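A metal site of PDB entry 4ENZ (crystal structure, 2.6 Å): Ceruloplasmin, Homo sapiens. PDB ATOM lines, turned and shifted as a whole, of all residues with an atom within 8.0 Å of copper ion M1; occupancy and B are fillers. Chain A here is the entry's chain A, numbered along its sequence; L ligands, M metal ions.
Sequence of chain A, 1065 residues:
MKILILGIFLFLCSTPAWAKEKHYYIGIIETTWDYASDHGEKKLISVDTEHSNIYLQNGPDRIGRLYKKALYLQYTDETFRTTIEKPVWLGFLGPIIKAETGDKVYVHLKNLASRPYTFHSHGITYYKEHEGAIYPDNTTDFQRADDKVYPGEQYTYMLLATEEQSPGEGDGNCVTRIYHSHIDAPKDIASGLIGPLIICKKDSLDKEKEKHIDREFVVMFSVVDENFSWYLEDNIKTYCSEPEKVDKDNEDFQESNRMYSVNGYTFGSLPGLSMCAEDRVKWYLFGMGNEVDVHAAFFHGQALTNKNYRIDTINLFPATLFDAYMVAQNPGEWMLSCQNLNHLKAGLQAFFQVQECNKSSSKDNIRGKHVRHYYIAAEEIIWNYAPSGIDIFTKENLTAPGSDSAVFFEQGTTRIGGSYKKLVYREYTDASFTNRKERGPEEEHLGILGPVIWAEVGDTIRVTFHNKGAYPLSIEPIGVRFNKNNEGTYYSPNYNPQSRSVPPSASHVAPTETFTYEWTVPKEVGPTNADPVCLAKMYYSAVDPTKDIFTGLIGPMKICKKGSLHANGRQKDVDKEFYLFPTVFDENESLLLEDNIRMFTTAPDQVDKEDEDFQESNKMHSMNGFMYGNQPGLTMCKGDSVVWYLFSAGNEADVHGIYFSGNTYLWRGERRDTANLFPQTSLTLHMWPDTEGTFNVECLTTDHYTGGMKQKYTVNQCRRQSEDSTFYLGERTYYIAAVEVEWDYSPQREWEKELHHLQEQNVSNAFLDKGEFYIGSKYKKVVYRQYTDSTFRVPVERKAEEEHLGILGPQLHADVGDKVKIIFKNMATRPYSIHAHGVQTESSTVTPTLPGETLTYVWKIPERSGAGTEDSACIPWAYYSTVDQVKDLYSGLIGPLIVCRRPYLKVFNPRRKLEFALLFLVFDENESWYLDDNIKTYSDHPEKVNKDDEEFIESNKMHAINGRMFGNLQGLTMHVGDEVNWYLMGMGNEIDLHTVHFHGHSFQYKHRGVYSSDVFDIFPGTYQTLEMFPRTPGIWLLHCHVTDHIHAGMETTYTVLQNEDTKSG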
ATOM      1  N   HIS A 120      -6.455   0.681 -15.857  1.00  0.00           N
ATOM      2  CA  HIS A 120      -5.717  -0.245 -16.702  1.00  0.00           C
ATOM      3  C   HIS A 120      -4.809   0.546 -17.598  1.00  0.00           C
ATOM      4  O   HIS A 120      -5.263   1.506 -18.205  1.00  0.00           O
ATOM      5  CB  HIS A 120      -6.698  -0.982 -17.558  1.00  0.00           C
ATOM      6  CG  HIS A 120      -6.072  -1.792 -18.646  1.00  0.00           C
ATOM      7  ND1 HIS A 120      -5.320  -2.918 -18.389  1.00  0.00           N
ATOM      8  CD2 HIS A 120      -6.109  -1.666 -19.989  1.00  0.00           C
ATOM      9  CE1 HIS A 120      -4.920  -3.442 -19.534  1.00  0.00           C
ATOM     10  NE2 HIS A 120      -5.403  -2.703 -20.514  1.00  0.00           N
ATOM     11  N   HIS A 122      -1.915   0.812 -20.783  1.00  0.00           N
ATOM     12  CA  HIS A 122      -1.561   0.119 -21.993  1.00  0.00           C
ATOM     13  C   HIS A 122      -0.054  -0.240 -22.123  1.00  0.00           C
ATOM     14  O   HIS A 122       0.272  -1.400 -22.402  1.00  0.00           O
ATOM     15  CB  HIS A 122      -2.092   0.845 -23.231  1.00  0.00           C
ATOM     16  CG  HIS A 122      -3.508   0.487 -23.603  1.00  0.00           C
ATOM     17  ND1 HIS A 122      -3.856   0.070 -24.863  1.00  0.00           N
ATOM     18  CD2 HIS A 122      -4.658   0.488 -22.873  1.00  0.00           C
ATOM     19  CE1 HIS A 122      -5.159  -0.157 -24.912  1.00  0.00           C
ATOM     20  NE2 HIS A 122      -5.673   0.086 -23.719  1.00  0.00           N
ATOM     21  N   TYR A 126       2.893  -5.464 -15.917  1.00  0.00           N
ATOM     22  CA  TYR A 126       2.270  -5.691 -14.637  1.00  0.00           C
ATOM     23  C   TYR A 126       1.880  -7.128 -14.464  1.00  0.00           C
ATOM     24  O   TYR A 126       1.603  -7.814 -15.440  1.00  0.00           O
ATOM     25  CB  TYR A 126       1.028  -4.835 -14.486  1.00  0.00           C
ATOM     26  CG  TYR A 126       0.239  -4.675 -15.738  1.00  0.00           C
ATOM     27  CD1 TYR A 126      -0.429  -5.754 -16.311  1.00  0.00           C
ATOM     28  CD2 TYR A 126       0.124  -3.431 -16.367  1.00  0.00           C
ATOM     29  CE1 TYR A 126      -1.188  -5.605 -17.471  1.00  0.00           C
ATOM     30  CE2 TYR A 126      -0.639  -3.277 -17.536  1.00  0.00           C
ATOM     31  CZ  TYR A 126      -1.284  -4.385 -18.074  1.00  0.00           C
ATOM     32  OH  TYR A 126      -2.032  -4.293 -19.235  1.00  0.00           O
ATOM     33  N   GLU A 131      -3.348  -5.221 -13.396  1.00  0.00           N
ATOM     34  CA  GLU A 131      -3.855  -5.006 -14.753  1.00  0.00           C
ATOM     35  C   GLU A 131      -5.064  -4.081 -14.775  1.00  0.00           C
ATOM     36  O   GLU A 131      -5.333  -3.430 -15.752  1.00  0.00           O
ATOM     37  CB  GLU A 131      -4.285  -6.377 -15.352  1.00  0.00           C
ATOM     38  CG  GLU A 131      -4.848  -6.378 -16.772  1.00  0.00           C
ATOM     39  CD  GLU A 131      -5.251  -7.791 -17.233  1.00  0.00           C
ATOM     40  OE1 GLU A 131      -5.331  -8.732 -16.394  1.00  0.00           O
ATOM     41  OE2 GLU A 131      -5.517  -7.945 -18.452  1.00  0.00           O
ATOM     42  N   ALA A 133      -8.293  -4.743 -15.016  1.00  0.00           N
ATOM     43  CA  ALA A 133      -9.287  -5.081 -16.008  1.00  0.00           C
ATOM     44  C   ALA A 133      -9.971  -6.405 -15.615  1.00  0.00           C
ATOM     45  O   ALA A 133      -9.315  -7.362 -15.208  1.00  0.00           O
ATOM     46  CB  ALA A 133      -8.651  -5.159 -17.383  1.00  0.00           C
ATOM     47  N   ILE A 134     -11.303  -6.430 -15.722  1.00  0.00           N
ATOM     48  CA  ILE A 134     -12.089  -7.542 -15.262  1.00  0.00           C
ATOM     49  C   ILE A 134     -12.527  -8.375 -16.437  1.00  0.00           C
ATOM     50  O   ILE A 134     -13.006  -7.865 -17.426  1.00  0.00           O
ATOM     51  CB  ILE A 134     -13.311  -7.096 -14.429  1.00  0.00           C
ATOM     52  CG1 ILE A 134     -13.675  -8.174 -13.370  1.00  0.00           C
ATOM     53  CG2 ILE A 134     -14.497  -6.780 -15.330  1.00  0.00           C
ATOM     54  CD1 ILE A 134     -14.381  -7.646 -12.149  1.00  0.00           C
ATOM     55  N   TYR A 135     -12.309  -9.673 -16.341  1.00  0.00           N
ATOM     56  CA  TYR A 135     -12.694 -10.606 -17.399  1.00  0.00           C
ATOM     57  C   TYR A 135     -12.307 -11.999 -16.975  1.00  0.00           C
ATOM     58  O   TYR A 135     -11.475 -12.147 -16.069  1.00  0.00           O
ATOM     59  CB  TYR A 135     -12.026 -10.274 -18.738  1.00  0.00           C
ATOM     60  CG  TYR A 135     -10.496 -10.232 -18.783  1.00  0.00           C
ATOM     61  CD1 TYR A 135      -9.826  -9.037 -18.700  1.00  0.00           C
ATOM     62  CD2 TYR A 135      -9.738 -11.384 -18.989  1.00  0.00           C
ATOM     63  CE1 TYR A 135      -8.426  -8.980 -18.815  1.00  0.00           C
ATOM     64  CE2 TYR A 135      -8.334 -11.348 -19.081  1.00  0.00           C
ATOM     65  CZ  TYR A 135      -7.690 -10.139 -19.003  1.00  0.00           C
ATOM     66  OH  TYR A 135      -6.330 -10.052 -19.120  1.00  0.00           O
ATOM     67  N   HIS A 180      -6.968   3.689 -19.001  1.00  0.00           N
ATOM     68  CA  HIS A 180      -8.410   3.886 -18.869  1.00  0.00           C
ATOM     69  C   HIS A 180      -9.010   2.897 -17.889  1.00  0.00           C
ATOM     70  O   HIS A 180      -8.366   1.941 -17.512  1.00  0.00           O
ATOM     71  CB  HIS A 180      -9.113   3.766 -20.222  1.00  0.00           C
ATOM     72  CG  HIS A 180      -8.784   2.527 -21.018  1.00  0.00           C
ATOM     73  ND1 HIS A 180      -9.631   1.438 -21.085  1.00  0.00           N
ATOM     74  CD2 HIS A 180      -7.782   2.268 -21.892  1.00  0.00           C
ATOM     75  CE1 HIS A 180      -9.134   0.540 -21.919  1.00  0.00           C
ATOM     76  NE2 HIS A 180      -8.000   1.015 -22.418  1.00  0.00           N
ATOM     77  N   SER A 181     -10.256   3.123 -17.494  1.00  0.00           N
ATOM     78  CA  SER A 181     -10.936   2.159 -16.650  1.00  0.00           C
ATOM     79  C   SER A 181     -11.434   0.976 -17.518  1.00  0.00           C
ATOM     80  O   SER A 181     -11.700   1.164 -18.700  1.00  0.00           O
ATOM     81  CB  SER A 181     -12.059   2.844 -15.871  1.00  0.00           C
ATOM     82  OG  SER A 181     -12.759   1.920 -15.069  1.00  0.00           O
ATOM     83  N   HIS A 182     -11.483  -0.245 -16.952  1.00  0.00           N
ATOM     84  CA  HIS A 182     -11.694  -1.467 -17.759  1.00  0.00           C
ATOM     85  C   HIS A 182     -12.607  -2.462 -17.027  1.00  0.00           C
ATOM     86  O   HIS A 182     -12.245  -3.632 -16.797  1.00  0.00           O
ATOM     87  CB  HIS A 182     -10.354  -2.124 -18.184  1.00  0.00           C
ATOM     88  CG  HIS A 182     -10.453  -2.969 -19.428  1.00  0.00           C
ATOM     89  ND1 HIS A 182     -11.403  -3.951 -19.599  1.00  0.00           N
ATOM     90  CD2 HIS A 182      -9.697  -2.976 -20.569  1.00  0.00           C
ATOM     91  CE1 HIS A 182     -11.249  -4.512 -20.793  1.00  0.00           C
ATOM     92  NE2 HIS A 182     -10.218  -3.942 -21.401  1.00  0.00           N
ATOM     93  N   ALA A 185     -14.978  -1.141 -20.594  1.00  0.00           N
ATOM     94  CA  ALA A 185     -14.040  -0.109 -21.031  1.00  0.00           C
ATOM     95  C   ALA A 185     -14.740   0.921 -21.896  1.00  0.00           C
ATOM     96  O   ALA A 185     -14.686   2.109 -21.619  1.00  0.00           O
ATOM     97  CB  ALA A 185     -12.883  -0.703 -21.747  1.00  0.00           C
ATOM     98  N   PRO A 186     -15.449   0.481 -22.936  1.00  0.00           N
ATOM     99  CA  PRO A 186     -16.157   1.456 -23.755  1.00  0.00           C
ATOM    100  C   PRO A 186     -16.978   2.463 -22.950  1.00  0.00           C
ATOM    101  O   PRO A 186     -16.816   3.691 -23.155  1.00  0.00           O
ATOM    102  CB  PRO A 186     -17.076   0.588 -24.590  1.00  0.00           C
ATOM    103  CG  PRO A 186     -16.257  -0.630 -24.812  1.00  0.00           C
ATOM    104  CD  PRO A 186     -15.508  -0.868 -23.538  1.00  0.00           C
ATOM    105  N   HIS A 997      -5.452  -5.410 -29.965  1.00  0.00           N
ATOM    106  CA  HIS A 997      -4.746  -5.070 -28.760  1.00  0.00           C
ATOM    107  C   HIS A 997      -4.514  -6.271 -27.873  1.00  0.00           C
ATOM    108  O   HIS A 997      -5.454  -7.043 -27.643  1.00  0.00           O
ATOM    109  CB  HIS A 997      -5.574  -4.052 -28.007  1.00  0.00           C
ATOM    110  CG  HIS A 997      -4.972  -3.666 -26.692  1.00  0.00           C
ATOM    111  ND1 HIS A 997      -3.627  -3.436 -26.535  1.00  0.00           N
ATOM    112  CD2 HIS A 997      -5.529  -3.496 -25.484  1.00  0.00           C
ATOM    113  CE1 HIS A 997      -3.371  -3.140 -25.280  1.00  0.00           C
ATOM    114  NE2 HIS A 997      -4.516  -3.168 -24.618  1.00  0.00           N
ATOM    115  N   PHE A 998      -3.294  -6.411 -27.368  1.00  0.00           N
ATOM    116  CA  PHE A 998      -2.914  -7.522 -26.495  1.00  0.00           C
ATOM    117  C   PHE A 998      -2.700  -6.966 -25.108  1.00  0.00           C
ATOM    118  O   PHE A 998      -1.887  -6.060 -24.909  1.00  0.00           O
ATOM    119  CB  PHE A 998      -1.605  -8.156 -26.955  1.00  0.00           C
ATOM    120  CG  PHE A 998      -1.633  -8.768 -28.344  1.00  0.00           C
ATOM    121  CD1 PHE A 998      -1.863 -10.128 -28.518  1.00  0.00           C
ATOM    122  CD2 PHE A 998      -1.351  -7.996 -29.469  1.00  0.00           C
ATOM    123  CE1 PHE A 998      -1.858 -10.696 -29.798  1.00  0.00           C
ATOM    124  CE2 PHE A 998      -1.333  -8.550 -30.734  1.00  0.00           C
ATOM    125  CZ  PHE A 998      -1.610  -9.904 -30.909  1.00  0.00           C
ATOM    126  N   HIS A 999      -3.437  -7.487 -24.144  1.00  0.00           N
ATOM    127  CA  HIS A 999      -3.271  -7.072 -22.768  1.00  0.00           C
ATOM    128  C   HIS A 999      -1.979  -7.698 -22.241  1.00  0.00           C
ATOM    129  O   HIS A 999      -1.632  -8.848 -22.561  1.00  0.00           O
ATOM    130  CB  HIS A 999      -4.430  -7.593 -21.940  1.00  0.00           C
ATOM    131  CG  HIS A 999      -5.620  -6.695 -21.899  1.00  0.00           C
ATOM    132  ND1 HIS A 999      -6.153  -6.222 -20.713  1.00  0.00           N
ATOM    133  CD2 HIS A 999      -6.390  -6.175 -22.891  1.00  0.00           C
ATOM    134  CE1 HIS A 999      -7.189  -5.454 -20.976  1.00  0.00           C
ATOM    135  NE2 HIS A 999      -7.358  -5.408 -22.283  1.00  0.00           N
ATOM    136  N   LEU A1037      -6.266 -10.936 -22.016  1.00  0.00           N
ATOM    137  CA  LEU A1037      -7.284 -10.634 -22.999  1.00  0.00           C
ATOM    138  C   LEU A1037      -6.659 -10.109 -24.281  1.00  0.00           C
ATOM    139  O   LEU A1037      -5.667  -9.342 -24.266  1.00  0.00           O
ATOM    140  CB  LEU A1037      -8.243  -9.576 -22.412  1.00  0.00           C
ATOM    141  CG  LEU A1037      -9.609  -9.321 -23.071  1.00  0.00           C
ATOM    142  CD1 LEU A1037     -10.463 -10.559 -23.049  1.00  0.00           C
ATOM    143  CD2 LEU A1037     -10.345  -8.162 -22.352  1.00  0.00           C
ATOM    144  N   LEU A1038      -7.278 -10.540 -25.380  1.00  0.00           N
ATOM    145  CA  LEU A1038      -6.918 -10.107 -26.710  1.00  0.00           C
ATOM    146  C   LEU A1038      -8.184  -9.662 -27.390  1.00  0.00           C
ATOM    147  O   LEU A1038      -9.130 -10.411 -27.515  1.00  0.00           O
ATOM    148  CB  LEU A1038      -6.319 -11.276 -27.449  1.00  0.00           C
ATOM    149  CG  LEU A1038      -5.558 -11.095 -28.755  1.00  0.00           C
ATOM    150  CD1 LEU A1038      -5.012 -12.478 -29.112  1.00  0.00           C
ATOM    151  CD2 LEU A1038      -6.435 -10.551 -29.858  1.00  0.00           C
ATOM    152  N   HIS A1039      -8.191  -8.418 -27.845  1.00  0.00           N
ATOM    153  CA  HIS A1039      -9.386  -7.864 -28.444  1.00  0.00           C
ATOM    154  C   HIS A1039      -9.132  -6.690 -29.363  1.00  0.00           C
ATOM    155  O   HIS A1039      -8.069  -6.047 -29.326  1.00  0.00           O
ATOM    156  CB  HIS A1039     -10.390  -7.457 -27.360  1.00  0.00           C
ATOM    157  CG  HIS A1039      -9.971  -6.273 -26.518  1.00  0.00           C
ATOM    158  ND1 HIS A1039     -10.250  -4.961 -26.876  1.00  0.00           N
ATOM    159  CD2 HIS A1039      -9.381  -6.211 -25.286  1.00  0.00           C
ATOM    160  CE1 HIS A1039      -9.811  -4.155 -25.914  1.00  0.00           C
ATOM    161  NE2 HIS A1039      -9.279  -4.889 -24.941  1.00  0.00           N
ATOM    162  N   CYS A1040     -10.156  -6.412 -30.172  1.00  0.00           N
ATOM    163  CA  CYS A1040     -10.278  -5.178 -30.952  1.00  0.00           C
ATOM    164  C   CYS A1040     -10.778  -4.074 -30.035  1.00  0.00           C
ATOM    165  O   CYS A1040     -11.642  -4.324 -29.205  1.00  0.00           O
ATOM    166  CB  CYS A1040     -11.301  -5.384 -32.052  1.00  0.00           C
ATOM    167  SG  CYS A1040     -11.432  -3.983 -33.090  1.00  0.00           S
ATOM    168  N   HIS A1041     -10.258  -2.858 -30.171  1.00  0.00           N
ATOM    169  CA  HIS A1041     -10.562  -1.827 -29.196  1.00  0.00           C
ATOM    170  C   HIS A1041     -11.705  -0.963 -29.727  1.00  0.00           C
ATOM    171  O   HIS A1041     -12.028   0.031 -29.111  1.00  0.00           O
ATOM    172  CB  HIS A1041      -9.301  -0.976 -28.917  1.00  0.00           C
ATOM    173  CG  HIS A1041      -9.134  -0.475 -27.505  1.00  0.00           C
ATOM    174  ND1 HIS A1041      -9.874   0.554 -26.969  1.00  0.00           N
ATOM    175  CD2 HIS A1041      -8.187  -0.784 -26.568  1.00  0.00           C
ATOM    176  CE1 HIS A1041      -9.431   0.809 -25.746  1.00  0.00           C
ATOM    177  NE2 HIS A1041      -8.400   0.018 -25.482  1.00  0.00           N
ATOM    178  N   ILE A1046     -15.890  -4.810 -29.465  1.00  0.00           N
ATOM    179  CA  ILE A1046     -15.690  -5.502 -28.172  1.00  0.00           C
ATOM    180  C   ILE A1046     -17.013  -6.065 -27.703  1.00  0.00           C
ATOM    181  O   ILE A1046     -17.123  -7.222 -27.431  1.00  0.00           O
ATOM    182  CB  ILE A1046     -15.207  -4.599 -26.989  1.00  0.00           C
ATOM    183  CG1 ILE A1046     -14.034  -3.713 -27.379  1.00  0.00           C
ATOM    184  CG2 ILE A1046     -14.775  -5.496 -25.781  1.00  0.00           C
ATOM    185  CD1 ILE A1046     -13.439  -2.873 -26.196  1.00  0.00           C
ATOM    186  N   GLU A1051     -13.149 -10.852 -29.344  1.00  0.00           N
ATOM    187  CA  GLU A1051     -12.196 -10.957 -28.244  1.00  0.00           C
ATOM    188  C   GLU A1051     -11.959 -12.392 -27.839  1.00  0.00           C
ATOM    189  O   GLU A1051     -12.854 -13.215 -27.943  1.00  0.00           O
ATOM    190  CB  GLU A1051     -12.764 -10.252 -27.032  1.00  0.00           C
ATOM    191  CG  GLU A1051     -14.092 -10.841 -26.539  1.00  0.00           C
ATOM    192  CD  GLU A1051     -14.810  -9.903 -25.583  1.00  0.00           C
ATOM    193  OE1 GLU A1051     -14.102  -9.133 -24.872  1.00  0.00           O
ATOM    194  OE2 GLU A1051     -16.073  -9.925 -25.558  1.00  0.00           O
HETATM  195  O1  LIG L   1      -7.799  -2.003 -23.489  1.00  0.00           O
HETATM  196  O2  LIG L   1      -6.961  -2.789 -23.075  1.00  0.00           O
HETATM  197 CU    CU M   1      -8.990  -4.415 -23.042  1.00  0.00          CU
HETATM  198 CU    CU M   2      -4.804  -3.003 -22.494  1.00  0.00          CU
HETATM  199 CU    CU M   3      -7.368   0.245 -24.053  1.00  0.00          CU
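The backbone carbonyl oxygen of His 1039 is in hydrogen-bond range of the backbone NH of His 997 (2.8 Å).
O of Leu 1037 sits at hydrogen-bond distance from N of His 999 (2.9 Å).
The side-chain carboxylate (OE2) of Glu 131 is in hydrogen-bond range of a ring nitrogen (ND1) of His 999 (2.9 Å).
The backbone NH of Ile 134 sits at hydrogen-bond distance from the backbone carbonyl oxygen of His 182.
Three residues have an atom within 4 Å of copper ion M1: His 182, His 999 and His 1039.
The nearest printed residue that does not touch copper ion M1 is Leu 1037 (4.04 Å).
Copper ion M1 is bound by a ring nitrogen (NE2) of His 1039 (2.0 Å), a ring nitrogen (NE2) of His 999 (2.1 Å) and a ring nitrogen (NE2) of His 182 (2.1 Å).
Copper ion M1 has three donor atoms within binding distance.
Slightly farther from copper ion M1 lies O2 of the ligand (2.6 Å).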
